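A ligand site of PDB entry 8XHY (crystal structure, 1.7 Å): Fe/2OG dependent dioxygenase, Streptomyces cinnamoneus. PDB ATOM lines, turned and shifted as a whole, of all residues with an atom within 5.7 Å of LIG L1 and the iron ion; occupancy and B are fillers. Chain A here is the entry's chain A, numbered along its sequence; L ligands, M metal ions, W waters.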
ATOM      1  N   TRP A 116     -31.165  23.470 -27.938  1.00  0.00           N
ATOM      2  CA  TRP A 116     -31.485  22.061 -27.750  1.00  0.00           C
ATOM      3  C   TRP A 116     -32.981  21.852 -27.605  1.00  0.00           C
ATOM      4  O   TRP A 116     -33.713  22.719 -27.135  1.00  0.00           O
ATOM      5  CB  TRP A 116     -30.747  21.427 -26.572  1.00  0.00           C
ATOM      6  CG  TRP A 116     -30.911  21.986 -25.185  1.00  0.00           C
ATOM      7  CD1 TRP A 116     -31.740  22.988 -24.756  1.00  0.00           C
ATOM      8  CD2 TRP A 116     -30.165  21.555 -24.046  1.00  0.00           C
ATOM      9  NE1 TRP A 116     -31.542  23.212 -23.404  1.00  0.00           N
ATOM     10  CE2 TRP A 116     -30.594  22.327 -22.949  1.00  0.00           C
ATOM     11  CE3 TRP A 116     -29.185  20.576 -23.850  1.00  0.00           C
ATOM     12  CZ2 TRP A 116     -30.064  22.149 -21.654  1.00  0.00           C
ATOM     13  CZ3 TRP A 116     -28.660  20.383 -22.568  1.00  0.00           C
ATOM     14  CH2 TRP A 116     -29.107  21.165 -21.494  1.00  0.00           C
ATOM     15  N   TYR A 120     -36.330  13.176 -22.442  1.00  0.00           N
ATOM     16  CA  TYR A 120     -35.870  12.748 -21.131  1.00  0.00           C
ATOM     17  C   TYR A 120     -36.687  11.554 -20.666  1.00  0.00           C
ATOM     18  O   TYR A 120     -37.918  11.616 -20.663  1.00  0.00           O
ATOM     19  CB  TYR A 120     -36.028  13.874 -20.090  1.00  0.00           C
ATOM     20  CG  TYR A 120     -35.082  15.078 -20.192  1.00  0.00           C
ATOM     21  CD1 TYR A 120     -33.995  15.097 -21.056  1.00  0.00           C
ATOM     22  CD2 TYR A 120     -35.280  16.177 -19.390  1.00  0.00           C
ATOM     23  CE1 TYR A 120     -33.138  16.178 -21.128  1.00  0.00           C
ATOM     24  CE2 TYR A 120     -34.414  17.296 -19.448  1.00  0.00           C
ATOM     25  CZ  TYR A 120     -33.351  17.279 -20.309  1.00  0.00           C
ATOM     26  OH  TYR A 120     -32.491  18.373 -20.352  1.00  0.00           O
ATOM     27  N   ALA A 179     -31.146  10.995 -21.080  1.00  0.00           N
ATOM     28  CA  ALA A 179     -31.532  12.298 -21.590  1.00  0.00           C
ATOM     29  C   ALA A 179     -30.881  12.506 -22.935  1.00  0.00           C
ATOM     30  O   ALA A 179     -29.642  12.473 -23.023  1.00  0.00           O
ATOM     31  CB  ALA A 179     -31.092  13.395 -20.602  1.00  0.00           C
ATOM     32  N   ASN A 181     -30.191  14.948 -26.286  1.00  0.00           N
ATOM     33  CA  ASN A 181     -30.151  16.361 -26.667  1.00  0.00           C
ATOM     34  C   ASN A 181     -29.910  16.494 -28.156  1.00  0.00           C
ATOM     35  O   ASN A 181     -28.935  15.930 -28.674  1.00  0.00           O
ATOM     36  CB  ASN A 181     -29.014  17.110 -25.965  1.00  0.00           C
ATOM     37  CG  ASN A 181     -29.091  17.024 -24.468  1.00  0.00           C
ATOM     38  OD1 ASN A 181     -30.172  17.162 -23.871  1.00  0.00           O
ATOM     39  ND2 ASN A 181     -27.949  16.730 -23.823  1.00  0.00           N
ATOM     40  N   PHE A 183     -29.207  19.654 -30.689  1.00  0.00           N
ATOM     41  CA  PHE A 183     -28.984  21.087 -30.751  1.00  0.00           C
ATOM     42  C   PHE A 183     -29.453  21.567 -32.122  1.00  0.00           C
ATOM     43  O   PHE A 183     -28.855  21.218 -33.152  1.00  0.00           O
ATOM     44  CB  PHE A 183     -27.517  21.411 -30.473  1.00  0.00           C
ATOM     45  CG  PHE A 183     -27.134  21.059 -29.072  1.00  0.00           C
ATOM     46  CD1 PHE A 183     -26.665  19.784 -28.777  1.00  0.00           C
ATOM     47  CD2 PHE A 183     -27.272  21.971 -28.050  1.00  0.00           C
ATOM     48  CE1 PHE A 183     -26.334  19.395 -27.491  1.00  0.00           C
ATOM     49  CE2 PHE A 183     -26.955  21.612 -26.733  1.00  0.00           C
ATOM     50  CZ  PHE A 183     -26.451  20.305 -26.456  1.00  0.00           C
ATOM     51  N   SER A 192     -27.319  25.723 -25.015  1.00  0.00           N
ATOM     52  CA  SER A 192     -28.118  25.620 -23.801  1.00  0.00           C
ATOM     53  C   SER A 192     -27.879  26.897 -22.986  1.00  0.00           C
ATOM     54  O   SER A 192     -26.930  27.630 -23.223  1.00  0.00           O
ATOM     55  CB  SER A 192     -27.697  24.418 -22.947  1.00  0.00           C
ATOM     56  OG  SER A 192     -26.417  24.647 -22.362  1.00  0.00           O
ATOM     57  N   HIS A 195     -25.814  26.318 -16.892  1.00  0.00           N
ATOM     58  CA  HIS A 195     -26.582  25.651 -15.853  1.00  0.00           C
ATOM     59  C   HIS A 195     -25.662  24.757 -15.016  1.00  0.00           C
ATOM     60  O   HIS A 195     -24.567  24.393 -15.442  1.00  0.00           O
ATOM     61  CB  HIS A 195     -27.719  24.786 -16.464  1.00  0.00           C
ATOM     62  CG  HIS A 195     -27.215  23.654 -17.310  1.00  0.00           C
ATOM     63  ND1 HIS A 195     -26.867  23.787 -18.640  1.00  0.00           N
ATOM     64  CD2 HIS A 195     -26.985  22.360 -16.989  1.00  0.00           C
ATOM     65  CE1 HIS A 195     -26.462  22.626 -19.110  1.00  0.00           C
ATOM     66  NE2 HIS A 195     -26.534  21.738 -18.128  1.00  0.00           N
ATOM     67  N   ARG A 196     -26.119  24.444 -13.806  1.00  0.00           N
ATOM     68  CA  ARG A 196     -25.628  23.285 -13.086  1.00  0.00           C
ATOM     69  C   ARG A 196     -26.627  22.148 -13.253  1.00  0.00           C
ATOM     70  O   ARG A 196     -27.846  22.371 -13.303  1.00  0.00           O
ATOM     71  CB  ARG A 196     -25.440  23.565 -11.592  1.00  0.00           C
ATOM     72  CG  ARG A 196     -24.313  24.574 -11.371  1.00  0.00           C
ATOM     73  CD  ARG A 196     -24.143  24.869  -9.859  1.00  0.00           C
ATOM     74  NE  ARG A 196     -25.042  25.938  -9.520  1.00  0.00           N
ATOM     75  CZ  ARG A 196     -24.708  27.061  -8.881  1.00  0.00           C
ATOM     76  NH1 ARG A 196     -23.464  27.257  -8.421  1.00  0.00           N
ATOM     77  NH2 ARG A 196     -25.649  27.954  -8.653  1.00  0.00           N
ATOM     78  N   ASP A 197     -26.115  20.940 -13.381  1.00  0.00           N
ATOM     79  CA  ASP A 197     -27.005  19.779 -13.362  1.00  0.00           C
ATOM     80  C   ASP A 197     -27.491  19.630 -11.927  1.00  0.00           C
ATOM     81  O   ASP A 197     -26.790  20.009 -10.996  1.00  0.00           O
ATOM     82  CB  ASP A 197     -26.288  18.501 -13.795  1.00  0.00           C
ATOM     83  CG  ASP A 197     -25.779  18.541 -15.248  1.00  0.00           C
ATOM     84  OD1 ASP A 197     -26.245  19.415 -16.015  1.00  0.00           O
ATOM     85  OD2 ASP A 197     -24.945  17.676 -15.622  1.00  0.00           O
ATOM     86  N   THR A 202     -23.305  13.105 -13.361  1.00  0.00           N
ATOM     87  CA  THR A 202     -23.788  13.080 -14.743  1.00  0.00           C
ATOM     88  C   THR A 202     -22.756  12.376 -15.616  1.00  0.00           C
ATOM     89  O   THR A 202     -21.568  12.705 -15.566  1.00  0.00           O
ATOM     90  CB  THR A 202     -24.005  14.508 -15.275  1.00  0.00           C
ATOM     91  OG1 THR A 202     -24.938  15.198 -14.430  1.00  0.00           O
ATOM     92  CG2 THR A 202     -24.562  14.504 -16.756  1.00  0.00           C
ATOM     93  N   LEU A 204     -21.779  11.761 -19.500  1.00  0.00           N
ATOM     94  CA  LEU A 204     -22.118  12.478 -20.731  1.00  0.00           C
ATOM     95  C   LEU A 204     -21.432  11.831 -21.922  1.00  0.00           C
ATOM     96  O   LEU A 204     -20.198  11.751 -21.967  1.00  0.00           O
ATOM     97  CB  LEU A 204     -21.703  13.958 -20.633  1.00  0.00           C
ATOM     98  CG  LEU A 204     -21.548  14.785 -21.929  1.00  0.00           C
ATOM     99  CD1 LEU A 204     -22.847  15.031 -22.663  1.00  0.00           C
ATOM    100  CD2 LEU A 204     -20.853  16.143 -21.623  1.00  0.00           C
ATOM    101  N   SER A 206     -20.701  12.500 -25.654  1.00  0.00           N
ATOM    102  CA  SER A 206     -20.631  13.496 -26.716  1.00  0.00           C
ATOM    103  C   SER A 206     -19.387  13.212 -27.532  1.00  0.00           C
ATOM    104  O   SER A 206     -18.462  12.526 -27.069  1.00  0.00           O
ATOM    105  CB  SER A 206     -20.578  14.925 -26.140  1.00  0.00           C
ATOM    106  OG  SER A 206     -19.449  15.029 -25.302  1.00  0.00           O
ATOM    107  N   GLY A 210     -17.969  22.070 -28.027  1.00  0.00           N
ATOM    108  CA  GLY A 210     -19.019  23.051 -27.825  1.00  0.00           C
ATOM    109  C   GLY A 210     -19.456  23.188 -26.382  1.00  0.00           C
ATOM    110  O   GLY A 210     -20.150  24.144 -25.998  1.00  0.00           O
ATOM    111  N   LEU A 211     -19.011  22.258 -25.527  1.00  0.00           N
ATOM    112  CA  LEU A 211     -19.345  22.397 -24.115  1.00  0.00           C
ATOM    113  C   LEU A 211     -18.340  23.377 -23.477  1.00  0.00           C
ATOM    114  O   LEU A 211     -17.135  23.231 -23.689  1.00  0.00           O
ATOM    115  CB  LEU A 211     -19.333  21.033 -23.411  1.00  0.00           C
ATOM    116  CG  LEU A 211     -19.545  21.054 -21.894  1.00  0.00           C
ATOM    117  CD1 LEU A 211     -20.904  21.679 -21.435  1.00  0.00           C
ATOM    118  CD2 LEU A 211     -19.384  19.604 -21.382  1.00  0.00           C
ATOM    119  N   ASN A 232     -19.416  14.888 -14.787  1.00  0.00           N
ATOM    120  CA  ASN A 232     -19.419  16.047 -13.906  1.00  0.00           C
ATOM    121  C   ASN A 232     -20.359  15.780 -12.741  1.00  0.00           C
ATOM    122  O   ASN A 232     -20.999  14.724 -12.632  1.00  0.00           O
ATOM    123  CB  ASN A 232     -19.765  17.352 -14.635  1.00  0.00           C
ATOM    124  CG  ASN A 232     -21.133  17.322 -15.273  1.00  0.00           C
ATOM    125  OD1 ASN A 232     -21.260  16.952 -16.424  1.00  0.00           O
ATOM    126  ND2 ASN A 232     -22.145  17.775 -14.550  1.00  0.00           N
ATOM    127  N   HIS A 253     -22.022  25.141 -16.587  1.00  0.00           N
ATOM    128  CA  HIS A 253     -21.559  24.762 -17.924  1.00  0.00           C
ATOM    129  C   HIS A 253     -22.698  24.966 -18.904  1.00  0.00           C
ATOM    130  O   HIS A 253     -23.869  25.023 -18.518  1.00  0.00           O
ATOM    131  CB  HIS A 253     -21.054  23.294 -17.930  1.00  0.00           C
ATOM    132  CG  HIS A 253     -22.112  22.301 -17.557  1.00  0.00           C
ATOM    133  ND1 HIS A 253     -22.511  22.080 -16.252  1.00  0.00           N
ATOM    134  CD2 HIS A 253     -22.929  21.546 -18.325  1.00  0.00           C
ATOM    135  CE1 HIS A 253     -23.475  21.186 -16.229  1.00  0.00           C
ATOM    136  NE2 HIS A 253     -23.741  20.841 -17.480  1.00  0.00           N
ATOM    137  N   GLY A 254     -22.352  25.030 -20.198  1.00  0.00           N
ATOM    138  CA  GLY A 254     -23.410  25.177 -21.198  1.00  0.00           C
ATOM    139  C   GLY A 254     -22.793  25.006 -22.557  1.00  0.00           C
ATOM    140  O   GLY A 254     -21.576  24.971 -22.715  1.00  0.00           O
ATOM    141  N   VAL A 255     -23.655  24.886 -23.562  1.00  0.00           N
ATOM    142  CA  VAL A 255     -23.201  24.586 -24.912  1.00  0.00           C
ATOM    143  C   VAL A 255     -23.291  25.834 -25.770  1.00  0.00           C
ATOM    144  O   VAL A 255     -24.295  26.579 -25.728  1.00  0.00           O
ATOM    145  CB  VAL A 255     -24.017  23.432 -25.521  1.00  0.00           C
ATOM    146  CG1 VAL A 255     -23.615  23.183 -26.995  1.00  0.00           C
ATOM    147  CG2 VAL A 255     -23.744  22.190 -24.720  1.00  0.00           C
ATOM    148  N   ARG A 267     -25.189  19.028 -33.959  1.00  0.00           N
ATOM    149  CA  ARG A 267     -24.611  18.485 -32.733  1.00  0.00           C
ATOM    150  C   ARG A 267     -25.678  17.773 -31.919  1.00  0.00           C
ATOM    151  O   ARG A 267     -26.821  18.224 -31.836  1.00  0.00           O
ATOM    152  CB  ARG A 267     -23.992  19.621 -31.905  1.00  0.00           C
ATOM    153  CG  ARG A 267     -23.162  19.094 -30.706  1.00  0.00           C
ATOM    154  CD  ARG A 267     -22.512  20.290 -29.989  1.00  0.00           C
ATOM    155  NE  ARG A 267     -21.541  19.850 -28.965  1.00  0.00           N
ATOM    156  CZ  ARG A 267     -21.877  19.410 -27.748  1.00  0.00           C
ATOM    157  NH1 ARG A 267     -23.146  19.364 -27.354  1.00  0.00           N
ATOM    158  NH2 ARG A 267     -20.912  18.995 -26.925  1.00  0.00           N
ATOM    159  N   THR A 268     -25.324  16.640 -31.335  1.00  0.00           N
ATOM    160  CA  THR A 268     -26.208  15.968 -30.398  1.00  0.00           C
ATOM    161  C   THR A 268     -25.360  15.543 -29.214  1.00  0.00           C
ATOM    162  O   THR A 268     -24.125  15.529 -29.260  1.00  0.00           O
ATOM    163  CB  THR A 268     -26.930  14.752 -31.008  1.00  0.00           C
ATOM    164  OG1 THR A 268     -25.969  13.729 -31.307  1.00  0.00           O
ATOM    165  CG2 THR A 268     -27.669  15.143 -32.324  1.00  0.00           C
ATOM    166  N   SER A 269     -26.037  15.187 -28.129  1.00  0.00           N
ATOM    167  CA  SER A 269     -25.349  14.521 -27.023  1.00  0.00           C
ATOM    168  C   SER A 269     -26.408  13.783 -26.229  1.00  0.00           C
ATOM    169  O   SER A 269     -27.603  14.036 -26.415  1.00  0.00           O
ATOM    170  CB  SER A 269     -24.612  15.488 -26.122  1.00  0.00           C
ATOM    171  OG  SER A 269     -25.478  16.471 -25.533  1.00  0.00           O
ATOM    172  N   VAL A 271     -26.968  11.882 -22.011  1.00  0.00           N
ATOM    173  CA  VAL A 271     -26.409  11.769 -20.659  1.00  0.00           C
ATOM    174  C   VAL A 271     -27.301  10.850 -19.854  1.00  0.00           C
ATOM    175  O   VAL A 271     -28.470  10.639 -20.191  1.00  0.00           O
ATOM    176  CB  VAL A 271     -26.306  13.112 -19.885  1.00  0.00           C
ATOM    177  CG1 VAL A 271     -25.581  14.150 -20.676  1.00  0.00           C
ATOM    178  CG2 VAL A 271     -27.671  13.592 -19.506  1.00  0.00           C
ATOM    179  N   PHE A 273     -28.508  11.386 -16.017  1.00  0.00           N
ATOM    180  CA  PHE A 273     -28.560  12.186 -14.791  1.00  0.00           C
ATOM    181  C   PHE A 273     -28.952  11.275 -13.629  1.00  0.00           C
ATOM    182  O   PHE A 273     -29.960  10.551 -13.717  1.00  0.00           O
ATOM    183  CB  PHE A 273     -29.611  13.295 -14.899  1.00  0.00           C
ATOM    184  CG  PHE A 273     -29.364  14.328 -15.976  1.00  0.00           C
ATOM    185  CD1 PHE A 273     -28.237  15.178 -15.928  1.00  0.00           C
ATOM    186  CD2 PHE A 273     -30.331  14.546 -16.974  1.00  0.00           C
ATOM    187  CE1 PHE A 273     -28.053  16.171 -16.876  1.00  0.00           C
ATOM    188  CE2 PHE A 273     -30.146  15.571 -17.961  1.00  0.00           C
ATOM    189  CZ  PHE A 273     -29.005  16.393 -17.885  1.00  0.00           C
HETATM  190  C1  LIG L   1     -26.725  18.513 -20.255  1.00  0.00           C
HETATM  191  O1  LIG L   1     -27.425  17.676 -20.927  1.00  0.00           O
HETATM  192  O2  LIG L   1     -27.067  18.842 -19.098  1.00  0.00           O
HETATM  193  C2  LIG L   1     -25.478  19.085 -20.795  1.00  0.00           C
HETATM  194  O3  LIG L   1     -24.804  19.900 -20.137  1.00  0.00           O
HETATM  195  C3  LIG L   1     -25.017  18.664 -22.175  1.00  0.00           C
HETATM  196  C4  LIG L   1     -23.552  18.981 -22.442  1.00  0.00           C
HETATM  197  C5  LIG L   1     -23.152  18.722 -23.888  1.00  0.00           C
HETATM  198  O4  LIG L   1     -24.014  18.520 -24.749  1.00  0.00           O
HETATM  199  O5  LIG L   1     -21.923  18.729 -24.193  1.00  0.00           O
HETATM  200  C1  LG2 L   2     -34.361  17.445 -13.388  1.00  0.00           C
HETATM  201  C2  LG2 L   2     -34.843  15.115 -12.646  1.00  0.00           C
HETATM  202  C3  LG2 L   2     -31.098  18.547 -16.039  1.00  0.00           C
HETATM  203  C4  LG2 L   2     -30.857  17.942 -14.677  1.00  0.00           C
HETATM  204  C5  LG2 L   2     -33.322  17.171 -14.522  1.00  0.00           C
HETATM  205  C6  LG2 L   2     -33.599  18.081 -15.732  1.00  0.00           C
HETATM  206  C7  LG2 L   2     -30.281  19.844 -16.231  1.00  0.00           C
HETATM  207  C8  LG2 L   2     -30.035  20.138 -17.803  1.00  0.00           C
HETATM  208  C9  LG2 L   2     -31.018  20.993 -15.576  1.00  0.00           C
HETATM  209  C10 LG2 L   2     -31.357  20.915 -13.999  1.00  0.00           C
HETATM  210  C11 LG2 L   2     -34.166  16.438 -12.198  1.00  0.00           C
HETATM  211  C12 LG2 L   2     -34.826  16.991 -10.919  1.00  0.00           C
HETATM  212  N1  LG2 L   2     -32.534  18.701 -16.372  1.00  0.00           N
HETATM  213  N2  LG2 L   2     -31.912  17.302 -14.015  1.00  0.00           N
HETATM  214  O1  LG2 L   2     -34.726  18.270 -16.146  1.00  0.00           O
HETATM  215  O2  LG2 L   2     -29.732  17.983 -14.173  1.00  0.00           O
HETATM  216 FE    FE M   1     -25.530  19.845 -18.084  1.00  0.00          FE
HETATM  217  O   HOH W   1     -24.486  17.963 -18.050  1.00  0.00           O
HETATM  218  O   HOH W   2     -30.097  17.374 -21.129  1.00  0.00           O
HETATM  219  O   HOH W   3     -19.414  17.606 -24.524  1.00  0.00           O
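The iron ion is bound by an oxygen (O2) of LIG L1 (2.1 Å), a ring nitrogen (NE2) of His 253 (2.1 Å), a ring nitrogen (NE2) of His 195 (2.1 Å), water W1 (2.2 Å), an oxygen (O3) of LIG L1 (2.2 Å) and the side-chain carboxylate (OD1) of Asp 197 (2.2 Å).
The iron ion has six donor atoms within binding distance.
The side-chain carboxylate of Asp 197 lies within hydrogen-bond range of the side-chain amide nitrogen of Asn 232 (3.0 Å).
The side-chain carboxylate (OD2) of Asp 197 sits at hydrogen-bond distance from the side-chain hydroxyl (OG1) of Thr 202 (2.7 Å).
The backbone carbonyl oxygen (O) of Ser 269 sits at hydrogen-bond distance from the backbone NH (N) of Asn 181 (2.7 Å).
The backbone carbonyl oxygen (O) of Arg 267 is in hydrogen-bond range of the backbone NH (N) of Phe 183, at 3.0 Å.
The side-chain hydroxyl (OG) of Ser 192 sits at hydrogen-bond distance from the backbone NH (N) of Val 255 (3.0 Å).
The backbone NH (N) of Ala 179 sits at hydrogen-bond distance from the backbone carbonyl oxygen (O) of Val 271 (2.8 Å).
Within 4 Å of the iron ion: His 195, Asp 197 and His 253.
The nearest printed residue that does not touch the iron ion is Phe 273 (4.6 Å).
OG of Ser 269 sits at hydrogen-bond distance from O4 of LIG L1 (2.6 Å).
An oxygen (O4) of LIG L1 lies within salt-bridge range of the guanidinium group (NH1) of Arg 267, at 2.9 Å.
The side-chain amide nitrogen (ND2) of Asn 181 is in hydrogen-bond range of an oxygen (O1) of LIG L1 (3.1 Å).
Trp 116 touches LIG L1.
Phe 183 touches LIG L1 (CZ to O4, 3.5 Å).
Leu 204 touches LIG L1 (CD2 to O5, 3.8 Å).
CB of Leu 211 touches O5 of LIG L1, 3.6 Å away.
Val 255 touches LIG L1.
Val 271 touches LIG L1.
CZ of Phe 273 touches O2 of LIG L1, at 3.4 Å.
Hydrophobic or aromatic side chains that line LIG L1: Trp 116, Phe 183, His 195, Leu 204, Leu 211, His 253, Val 255, Val 271 and Phe 273.
Of the 23 residues printed, 13 come within 4 Å of LIG L1.
Water W2 lies within hydrogen-bond range of an oxygen (O1) of LIG L1 (2.7 Å), the side-chain hydroxyl (OH) of Tyr 120 (2.7 Å) and the side-chain amide oxygen (OD1) of Asn 181 (2.8 Å).
Water W3 lies within hydrogen-bond range of OG of Ser 206, O5 of LIG L1 and NH2 of Arg 267.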
